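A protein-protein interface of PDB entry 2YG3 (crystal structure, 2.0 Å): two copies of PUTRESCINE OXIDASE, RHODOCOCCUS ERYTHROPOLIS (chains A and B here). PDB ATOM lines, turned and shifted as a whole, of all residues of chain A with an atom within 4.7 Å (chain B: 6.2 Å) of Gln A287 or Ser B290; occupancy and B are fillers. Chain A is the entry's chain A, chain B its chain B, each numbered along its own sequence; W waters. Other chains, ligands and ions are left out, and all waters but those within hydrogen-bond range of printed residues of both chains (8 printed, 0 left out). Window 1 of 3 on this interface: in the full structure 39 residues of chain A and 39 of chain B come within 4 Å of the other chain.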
ATOM      1  N   HIS A 283     -15.866  -8.947   3.702  1.00  0.00           N
ATOM      2  CA  HIS A 283     -15.874 -10.067   4.652  1.00  0.00           C
ATOM      3  C   HIS A 283     -16.406 -11.359   3.988  1.00  0.00           C
ATOM      4  O   HIS A 283     -15.841 -12.442   4.151  1.00  0.00           O
ATOM      5  CB  HIS A 283     -16.758  -9.785   5.876  1.00  0.00           C
ATOM      6  CG  HIS A 283     -16.120  -8.959   6.953  1.00  0.00           C
ATOM      7  ND1 HIS A 283     -14.760  -8.718   7.032  1.00  0.00           N
ATOM      8  CD2 HIS A 283     -16.668  -8.349   8.029  1.00  0.00           C
ATOM      9  CE1 HIS A 283     -14.504  -7.986   8.105  1.00  0.00           C
ATOM     10  NE2 HIS A 283     -15.644  -7.763   8.733  1.00  0.00           N
ATOM     11  N   GLN A 284     -17.509 -11.230   3.264  1.00  0.00           N
ATOM     12  CA  GLN A 284     -18.141 -12.347   2.584  1.00  0.00           C
ATOM     13  C   GLN A 284     -17.382 -12.785   1.321  1.00  0.00           C
ATOM     14  O   GLN A 284     -17.069 -13.972   1.144  1.00  0.00           O
ATOM     15  CB  GLN A 284     -19.584 -11.961   2.234  1.00  0.00           C
ATOM     16  CG  GLN A 284     -20.551 -12.092   3.439  1.00  0.00           C
ATOM     17  CD  GLN A 284     -21.113 -13.516   3.575  1.00  0.00           C
ATOM     18  OE1 GLN A 284     -21.000 -14.166   4.639  1.00  0.00           O
ATOM     19  NE2 GLN A 284     -21.708 -14.007   2.500  1.00  0.00           N
ATOM     20  N   MET A 285     -17.116 -11.838   0.430  1.00  0.00           N
ATOM     21  CA  MET A 285     -16.470 -12.175  -0.856  1.00  0.00           C
ATOM     22  C   MET A 285     -15.130 -12.874  -0.645  1.00  0.00           C
ATOM     23  O   MET A 285     -14.815 -13.856  -1.320  1.00  0.00           O
ATOM     24  CB  MET A 285     -16.268 -10.915  -1.699  1.00  0.00           C
ATOM     25  CG  MET A 285     -15.327 -11.083  -2.899  1.00  0.00           C
ATOM     26  SD  MET A 285     -15.241  -9.580  -3.911  1.00  0.00           S
ATOM     27  CE  MET A 285     -14.839  -8.327  -2.700  1.00  0.00           C
ATOM     28  N   HIS A 286     -14.323 -12.364   0.281  1.00  0.00           N
ATOM     29  CA  HIS A 286     -12.978 -12.918   0.470  1.00  0.00           C
ATOM     30  C   HIS A 286     -12.991 -14.382   0.933  1.00  0.00           C
ATOM     31  O   HIS A 286     -12.039 -15.120   0.657  1.00  0.00           O
ATOM     32  CB  HIS A 286     -12.164 -12.068   1.445  1.00  0.00           C
ATOM     33  CG  HIS A 286     -11.912 -10.676   0.956  1.00  0.00           C
ATOM     34  ND1 HIS A 286     -11.494  -9.658   1.791  1.00  0.00           N
ATOM     35  CD2 HIS A 286     -12.042 -10.128  -0.279  1.00  0.00           C
ATOM     36  CE1 HIS A 286     -11.350  -8.548   1.085  1.00  0.00           C
ATOM     37  NE2 HIS A 286     -11.685  -8.803  -0.173  1.00  0.00           N
ATOM     38  N   GLN A 287     -14.076 -14.815   1.588  1.00  0.00           N
ATOM     39  CA  GLN A 287     -14.196 -16.229   1.985  1.00  0.00           C
ATOM     40  C   GLN A 287     -14.436 -17.171   0.807  1.00  0.00           C
ATOM     41  O   GLN A 287     -14.211 -18.382   0.923  1.00  0.00           O
ATOM     42  CB  GLN A 287     -15.339 -16.435   2.986  1.00  0.00           C
ATOM     43  CG  GLN A 287     -15.123 -15.768   4.305  1.00  0.00           C
ATOM     44  CD  GLN A 287     -16.336 -15.912   5.182  1.00  0.00           C
ATOM     45  OE1 GLN A 287     -16.714 -17.027   5.549  1.00  0.00           O
ATOM     46  NE2 GLN A 287     -16.961 -14.793   5.518  1.00  0.00           N
ATOM     47  N   HIS A 288     -14.921 -16.628  -0.307  1.00  0.00           N
ATOM     48  CA  HIS A 288     -15.263 -17.467  -1.453  1.00  0.00           C
ATOM     49  C   HIS A 288     -14.149 -17.581  -2.505  1.00  0.00           C
ATOM     50  O   HIS A 288     -14.394 -18.070  -3.614  1.00  0.00           O
ATOM     51  CB  HIS A 288     -16.564 -16.978  -2.093  1.00  0.00           C
ATOM     52  CG  HIS A 288     -17.767 -17.173  -1.224  1.00  0.00           C
ATOM     53  ND1 HIS A 288     -18.456 -18.366  -1.169  1.00  0.00           N
ATOM     54  CD2 HIS A 288     -18.378 -16.343  -0.344  1.00  0.00           C
ATOM     55  CE1 HIS A 288     -19.460 -18.255  -0.315  1.00  0.00           C
ATOM     56  NE2 HIS A 288     -19.432 -17.035   0.201  1.00  0.00           N
ATOM     57  N   GLN A 289     -12.949 -17.129  -2.147  1.00  0.00           N
ATOM     58  CA  GLN A 289     -11.762 -17.152  -3.022  1.00  0.00           C
ATOM     59  C   GLN A 289     -10.826 -18.208  -2.438  1.00  0.00           C
ATOM     60  O   GLN A 289     -10.564 -18.183  -1.224  1.00  0.00           O
ATOM     61  CB  GLN A 289     -11.048 -15.793  -2.982  1.00  0.00           C
ATOM     62  CG  GLN A 289     -11.762 -14.587  -3.661  1.00  0.00           C
ATOM     63  CD  GLN A 289     -11.348 -14.448  -5.119  1.00  0.00           C
ATOM     64  OE1 GLN A 289     -11.054 -15.451  -5.781  1.00  0.00           O
ATOM     65  NE2 GLN A 289     -11.302 -13.212  -5.620  1.00  0.00           N
ATOM     66  N   ASP A 400     -15.130 -20.035  -5.636  1.00  0.00           N
ATOM     67  CA  ASP A 400     -15.869 -21.284  -5.558  1.00  0.00           C
ATOM     68  C   ASP A 400     -17.032 -21.204  -6.551  1.00  0.00           C
ATOM     69  O   ASP A 400     -17.230 -20.172  -7.187  1.00  0.00           O
ATOM     70  CB  ASP A 400     -16.344 -21.553  -4.127  1.00  0.00           C
ATOM     71  CG  ASP A 400     -17.248 -20.444  -3.569  1.00  0.00           C
ATOM     72  OD1 ASP A 400     -17.583 -19.471  -4.292  1.00  0.00           O
ATOM     73  OD2 ASP A 400     -17.652 -20.567  -2.391  1.00  0.00           O
ATOM     74  N   LYS B 176     -26.690 -20.667   1.567  1.00  0.00           N
ATOM     75  CA  LYS B 176     -25.950 -20.518   0.316  1.00  0.00           C
ATOM     76  C   LYS B 176     -26.874 -21.000  -0.788  1.00  0.00           C
ATOM     77  O   LYS B 176     -27.730 -21.855  -0.533  1.00  0.00           O
ATOM     78  CB  LYS B 176     -24.696 -21.405   0.319  1.00  0.00           C
ATOM     79  CG  LYS B 176     -23.559 -20.903   1.224  1.00  0.00           C
ATOM     80  CD  LYS B 176     -22.453 -21.941   1.345  1.00  0.00           C
ATOM     81  CE  LYS B 176     -21.220 -21.351   2.055  1.00  0.00           C
ATOM     82  NZ  LYS B 176     -20.115 -22.372   2.062  1.00  0.00           N
ATOM     83  N   PRO B 266     -14.175 -21.886  10.979  1.00  0.00           N
ATOM     84  CA  PRO B 266     -12.963 -22.184  10.213  1.00  0.00           C
ATOM     85  C   PRO B 266     -12.527 -21.071   9.233  1.00  0.00           C
ATOM     86  O   PRO B 266     -11.330 -20.952   8.945  1.00  0.00           O
ATOM     87  CB  PRO B 266     -13.302 -23.518   9.508  1.00  0.00           C
ATOM     88  CG  PRO B 266     -14.770 -23.598   9.521  1.00  0.00           C
ATOM     89  CD  PRO B 266     -15.256 -22.847  10.711  1.00  0.00           C
ATOM     90  N   ASN B 267     -13.460 -20.231   8.781  1.00  0.00           N
ATOM     91  CA  ASN B 267     -13.101 -19.033   7.990  1.00  0.00           C
ATOM     92  C   ASN B 267     -12.214 -18.033   8.749  1.00  0.00           C
ATOM     93  O   ASN B 267     -11.642 -17.129   8.131  1.00  0.00           O
ATOM     94  CB  ASN B 267     -14.367 -18.300   7.489  1.00  0.00           C
ATOM     95  CG  ASN B 267     -15.208 -17.743   8.632  1.00  0.00           C
ATOM     96  OD1 ASN B 267     -15.642 -18.484   9.502  1.00  0.00           O
ATOM     97  ND2 ASN B 267     -15.411 -16.439   8.646  1.00  0.00           N
ATOM     98  N   HIS B 286      -8.504 -25.073   4.831  1.00  0.00           N
ATOM     99  CA  HIS B 286      -9.140 -23.902   5.447  1.00  0.00           C
ATOM    100  C   HIS B 286      -9.679 -22.877   4.432  1.00  0.00           C
ATOM    101  O   HIS B 286     -10.628 -22.175   4.733  1.00  0.00           O
ATOM    102  CB  HIS B 286      -8.229 -23.224   6.486  1.00  0.00           C
ATOM    103  CG  HIS B 286      -7.907 -24.112   7.656  1.00  0.00           C
ATOM    104  ND1 HIS B 286      -6.893 -23.838   8.546  1.00  0.00           N
ATOM    105  CD2 HIS B 286      -8.452 -25.292   8.052  1.00  0.00           C
ATOM    106  CE1 HIS B 286      -6.842 -24.797   9.461  1.00  0.00           C
ATOM    107  NE2 HIS B 286      -7.775 -25.694   9.179  1.00  0.00           N
ATOM    108  N   GLN B 287      -9.094 -22.828   3.239  1.00  0.00           N
ATOM    109  CA  GLN B 287      -9.534 -21.855   2.226  1.00  0.00           C
ATOM    110  C   GLN B 287     -10.865 -22.273   1.609  1.00  0.00           C
ATOM    111  O   GLN B 287     -11.544 -21.464   0.972  1.00  0.00           O
ATOM    112  CB  GLN B 287      -8.503 -21.748   1.098  1.00  0.00           C
ATOM    113  CG  GLN B 287      -7.145 -21.139   1.489  1.00  0.00           C
ATOM    114  CD  GLN B 287      -6.177 -21.163   0.321  1.00  0.00           C
ATOM    115  OE1 GLN B 287      -6.454 -20.593  -0.738  1.00  0.00           O
ATOM    116  NE2 GLN B 287      -5.041 -21.821   0.504  1.00  0.00           N
ATOM    117  N   HIS B 288     -11.210 -23.554   1.748  1.00  0.00           N
ATOM    118  CA  HIS B 288     -12.386 -24.099   1.097  1.00  0.00           C
ATOM    119  C   HIS B 288     -13.608 -24.106   2.019  1.00  0.00           C
ATOM    120  O   HIS B 288     -14.605 -24.704   1.689  1.00  0.00           O
ATOM    121  CB  HIS B 288     -12.100 -25.499   0.552  1.00  0.00           C
ATOM    122  CG  HIS B 288     -11.156 -25.511  -0.615  1.00  0.00           C
ATOM    123  ND1 HIS B 288     -11.572 -25.303  -1.912  1.00  0.00           N
ATOM    124  CD2 HIS B 288      -9.815 -25.682  -0.673  1.00  0.00           C
ATOM    125  CE1 HIS B 288     -10.529 -25.363  -2.724  1.00  0.00           C
ATOM    126  NE2 HIS B 288      -9.448 -25.598  -1.995  1.00  0.00           N
ATOM    127  N   GLN B 289     -13.508 -23.437   3.167  1.00  0.00           N
ATOM    128  CA  GLN B 289     -14.607 -23.310   4.146  1.00  0.00           C
ATOM    129  C   GLN B 289     -15.101 -21.870   4.097  1.00  0.00           C
ATOM    130  O   GLN B 289     -14.291 -20.948   4.172  1.00  0.00           O
ATOM    131  CB  GLN B 289     -14.073 -23.550   5.573  1.00  0.00           C
ATOM    132  CG  GLN B 289     -13.637 -24.998   5.887  1.00  0.00           C
ATOM    133  CD  GLN B 289     -14.778 -25.808   6.491  1.00  0.00           C
ATOM    134  OE1 GLN B 289     -15.946 -25.604   6.142  1.00  0.00           O
ATOM    135  NE2 GLN B 289     -14.457 -26.714   7.393  1.00  0.00           N
ATOM    136  N   SER B 290     -16.417 -21.667   3.987  1.00  0.00           N
ATOM    137  CA  SER B 290     -16.977 -20.316   4.038  1.00  0.00           C
ATOM    138  C   SER B 290     -18.338 -20.313   4.718  1.00  0.00           C
ATOM    139  O   SER B 290     -19.112 -21.274   4.605  1.00  0.00           O
ATOM    140  CB  SER B 290     -17.103 -19.731   2.627  1.00  0.00           C
ATOM    141  OG  SER B 290     -17.902 -20.588   1.816  1.00  0.00           O
ATOM    142  N   LEU B 291     -18.617 -19.226   5.422  1.00  0.00           N
ATOM    143  CA  LEU B 291     -19.926 -18.995   6.027  1.00  0.00           C
ATOM    144  C   LEU B 291     -20.965 -18.653   4.961  1.00  0.00           C
ATOM    145  O   LEU B 291     -20.646 -18.027   3.935  1.00  0.00           O
ATOM    146  CB  LEU B 291     -19.837 -17.840   7.031  1.00  0.00           C
ATOM    147  CG  LEU B 291     -18.946 -18.076   8.265  1.00  0.00           C
ATOM    148  CD1 LEU B 291     -18.809 -16.780   9.054  1.00  0.00           C
ATOM    149  CD2 LEU B 291     -19.530 -19.123   9.147  1.00  0.00           C
ATOM    150  N   GLY B 292     -22.208 -19.061   5.202  1.00  0.00           N
ATOM    151  CA  GLY B 292     -23.310 -18.569   4.390  1.00  0.00           C
ATOM    152  C   GLY B 292     -23.653 -17.125   4.743  1.00  0.00           C
ATOM    153  O   GLY B 292     -22.936 -16.467   5.503  1.00  0.00           O
ATOM    154  N   THR B 391     -17.154 -12.823  13.262  1.00  0.00           N
ATOM    155  CA  THR B 391     -17.995 -13.859  12.692  1.00  0.00           C
ATOM    156  C   THR B 391     -17.896 -13.892  11.155  1.00  0.00           C
ATOM    157  O   THR B 391     -17.334 -14.824  10.619  1.00  0.00           O
ATOM    158  CB  THR B 391     -19.487 -13.725  13.120  1.00  0.00           C
ATOM    159  OG1 THR B 391     -19.570 -13.611  14.548  1.00  0.00           O
ATOM    160  CG2 THR B 391     -20.279 -14.947  12.675  1.00  0.00           C
ATOM    161  N   ARG B 392     -18.473 -12.882  10.482  1.00  0.00           N
ATOM    162  CA  ARG B 392     -18.372 -12.646   9.019  1.00  0.00           C
ATOM    163  C   ARG B 392     -19.411 -13.368   8.145  1.00  0.00           C
ATOM    164  O   ARG B 392     -19.196 -13.556   6.929  1.00  0.00           O
ATOM    165  CB  ARG B 392     -16.945 -12.891   8.489  1.00  0.00           C
ATOM    166  CG  ARG B 392     -15.875 -12.083   9.225  1.00  0.00           C
ATOM    167  CD  ARG B 392     -14.491 -12.188   8.571  1.00  0.00           C
ATOM    168  NE  ARG B 392     -13.489 -11.502   9.401  1.00  0.00           N
ATOM    169  CZ  ARG B 392     -12.368 -10.939   8.946  1.00  0.00           C
ATOM    170  NH1 ARG B 392     -12.061 -10.987   7.650  1.00  0.00           N
ATOM    171  NH2 ARG B 392     -11.548 -10.328   9.797  1.00  0.00           N
ATOM    172  N   GLY B 393     -20.538 -13.748   8.740  1.00  0.00           N
ATOM    173  CA  GLY B 393     -21.594 -14.456   8.025  1.00  0.00           C
ATOM    174  C   GLY B 393     -22.542 -15.124   8.999  1.00  0.00           C
ATOM    175  O   GLY B 393     -22.384 -14.981  10.210  1.00  0.00           O
ATOM    176  N   ALA B 396     -23.543 -20.460   9.543  1.00  0.00           N
ATOM    177  CA  ALA B 396     -22.362 -21.264   9.799  1.00  0.00           C
ATOM    178  C   ALA B 396     -21.631 -21.618   8.521  1.00  0.00           C
ATOM    179  O   ALA B 396     -22.100 -21.311   7.419  1.00  0.00           O
ATOM    180  CB  ALA B 396     -22.751 -22.524  10.561  1.00  0.00           C
ATOM    181  N   ALA B 397     -20.474 -22.255   8.681  1.00  0.00           N
ATOM    182  CA  ALA B 397     -19.594 -22.530   7.557  1.00  0.00           C
ATOM    183  C   ALA B 397     -19.852 -23.899   6.933  1.00  0.00           C
ATOM    184  O   ALA B 397     -20.300 -24.829   7.603  1.00  0.00           O
ATOM    185  CB  ALA B 397     -18.143 -22.401   7.991  1.00  0.00           C
ATOM    186  N   SER B 398     -19.601 -23.995   5.635  1.00  0.00           N
ATOM    187  CA  SER B 398     -19.666 -25.256   4.921  1.00  0.00           C
ATOM    188  C   SER B 398     -18.594 -25.228   3.843  1.00  0.00           C
ATOM    189  O   SER B 398     -18.118 -24.151   3.444  1.00  0.00           O
ATOM    190  CB  SER B 398     -21.057 -25.449   4.288  1.00  0.00           C
ATOM    191  OG  SER B 398     -21.453 -24.301   3.549  1.00  0.00           O
ATOM    192  N   PHE B 399     -18.223 -26.406   3.356  1.00  0.00           N
ATOM    193  CA  PHE B 399     -17.276 -26.483   2.249  1.00  0.00           C
ATOM    194  C   PHE B 399     -17.861 -25.905   0.973  1.00  0.00           C
ATOM    195  O   PHE B 399     -19.094 -25.838   0.815  1.00  0.00           O
ATOM    196  CB  PHE B 399     -16.831 -27.923   2.008  1.00  0.00           C
ATOM    197  CG  PHE B 399     -15.822 -28.386   3.001  1.00  0.00           C
ATOM    198  CD1 PHE B 399     -14.506 -27.928   2.938  1.00  0.00           C
ATOM    199  CD2 PHE B 399     -16.200 -29.226   4.045  1.00  0.00           C
ATOM    200  CE1 PHE B 399     -13.558 -28.334   3.898  1.00  0.00           C
ATOM    201  CE2 PHE B 399     -15.263 -29.636   5.005  1.00  0.00           C
ATOM    202  CZ  PHE B 399     -13.947 -29.196   4.916  1.00  0.00           C
ATOM    203  N   ASP B 400     -16.966 -25.464   0.092  1.00  0.00           N
ATOM    204  CA  ASP B 400     -17.368 -25.176  -1.273  1.00  0.00           C
ATOM    205  C   ASP B 400     -17.690 -26.518  -1.952  1.00  0.00           C
ATOM    206  O   ASP B 400     -17.518 -27.588  -1.350  1.00  0.00           O
ATOM    207  CB  ASP B 400     -16.296 -24.374  -2.024  1.00  0.00           C
ATOM    208  CG  ASP B 400     -14.930 -25.058  -2.057  1.00  0.00           C
ATOM    209  OD1 ASP B 400     -14.767 -26.214  -1.578  1.00  0.00           O
ATOM    210  OD2 ASP B 400     -14.014 -24.436  -2.628  1.00  0.00           O
HETATM  211  O   HOH W   1     -16.357 -21.874   0.155  1.00  0.00           O
HETATM  212  O   HOH W   2     -10.555 -18.324   1.537  1.00  0.00           O
HETATM  213  O   HOH W   3     -13.272 -12.484   5.288  1.00  0.00           O
HETATM  214  O   HOH W   4     -11.962  -9.861   4.589  1.00  0.00           O
HETATM  215  O   HOH W   5     -21.679 -16.513   1.858  1.00  0.00           O
HETATM  216  O   HOH W   6     -12.307 -19.120   3.713  1.00  0.00           O
HETATM  217  O   HOH W   7     -19.590 -21.758  -0.983  1.00  0.00           O
HETATM  218  O   HOH W   8     -13.875 -20.845  -0.179  1.00  0.00           O
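The side-chain amide oxygen (OE1) of Gln A284 sits close to the backbone carbonyl oxygen (O) of Gly B292 (3.1 Å). N of Leu B291 lies within hydrogen-bond range of OE1 of Gln A287 (2.9 Å). The backbone carbonyl oxygen of Arg B392 is in hydrogen-bond range of the side-chain amide nitrogen of Gln A287 (2.9 Å). O of Arg B392 sits close to OE1 of Gln A284. The side-chain amide oxygen (OE1) of Gln A287 sits close to the side-chain amide nitrogen (ND2) of Asn B267, 3.4 Å away.
The side-chain amino group of Lys B176 sits at hydrogen-bond distance from the side-chain hydroxyl of Ser B290, at 2.9 Å. The backbone carbonyl oxygen (O) of Ala B396 sits at hydrogen-bond distance from the backbone NH (N) of Gly B292 (3.2 Å). The backbone carbonyl oxygen (O) of Thr B391 is in hydrogen-bond range of the side-chain amide nitrogen (ND2) of Asn B267 (3.2 Å). NE2 of Gln A287 is in hydrogen-bond range of O of His A283 (2.9 Å). The backbone carbonyl oxygen of Ser B290 lies within hydrogen-bond range of the backbone NH of Ser B398, 3.0 Å away. The side-chain carboxylate (OD2) of Asp A400 is in hydrogen-bond range of a ring nitrogen (ND1) of His A288 (2.6 Å).
Among the printed residues, pairs that only touch across the chains: Gln A284 with Gly B393 (3.4 Å), Asp A400 with Asp B400 (3.5 Å), His A288 with Ser B290 (3.5 Å), His A283 with Arg B392 (3.6 Å), Gln A287 with Ser B290 (3.6 Å) and Gln A284 with Leu B291 (3.9 Å).
Of chain B, only Asn B267 (3.3 Å), Ser B290 (3.6 Å), Leu B291 (2.9 Å) and Arg B392 (2.9 Å) come within 4 Å of Gln A287. Ser B290 touches just these residues of chain A: Gln A287 (3.6 Å) and His A288 (3.5 Å). Of the printed residues of chain A, Arg B392 touches His A283 (3.6 Å), Gln A284 (3.0 Å) and Gln A287 (2.9 Å). Printed residues of chain B within 4 Å of His A288: Ser B290 (3.5 Å). Printed residues of chain B within 4 Å of Gln A284: Leu B291, Gly B292, Arg B392 and Gly B393. Printed residues of chain A within 4 Å of Asp B400: Asp A400 (3.5 Å). Ala B396 touches none of the printed residues of chain A. The nearest printed residue of chain A that does not touch Arg B392 is His A286 (6.0 Å).
Of the 18 printed residues of chain B, 7 touch a printed residue of chain A. Printed residues of chain B that touch a printed residue of chain A: Asn B267, Ser B290, Leu B291, Gly B292, Arg B392, Gly B393 and Asp B400. Hydrophobic or aromatic side chains of chain B that line the printed part of chain A: Leu B291. Along chain B the printed residues that touch a printed residue of chain A span positions 267 to 400. Hydrophobic or aromatic side chains of chain A that line the printed part of chain B: His A283 and His A288. Among the printed residues, no Asp or Glu carboxylate lies within 4 Å of a Lys or Arg side-chain nitrogen of the other chain.
Asp A400 touches its own counterpart, Asp B400. 5 positions are printed for both chains.
Water W5 lies within hydrogen-bond range of the side-chain amide nitrogen (NE2) of Gln A284, the backbone carbonyl oxygen (O) of Leu B291 and a ring nitrogen (NE2) of His A288. Water W8 lies within hydrogen-bond range of the backbone carbonyl oxygen of Gln B287 (2.7 Å) and the backbone carbonyl oxygen of Gln A287 (2.7 Å). Water W7 lies within hydrogen-bond range of OD2 of Asp A400 (2.7 Å), NZ of Lys B176 (3.2 Å) and OG of Ser B290 (3.5 Å). Water W2 bridges the backbone carbonyl oxygen of Gln A289 and the backbone carbonyl oxygen of Gln B287. Water W3 bridges the backbone carbonyl oxygen (O) of His A283 (2.8 Å) and the guanidinium group (NH1) of Arg B392 (3.0 Å). Water W4 lies within hydrogen-bond range of ND1 of His A286 and NH1 of Arg B392.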
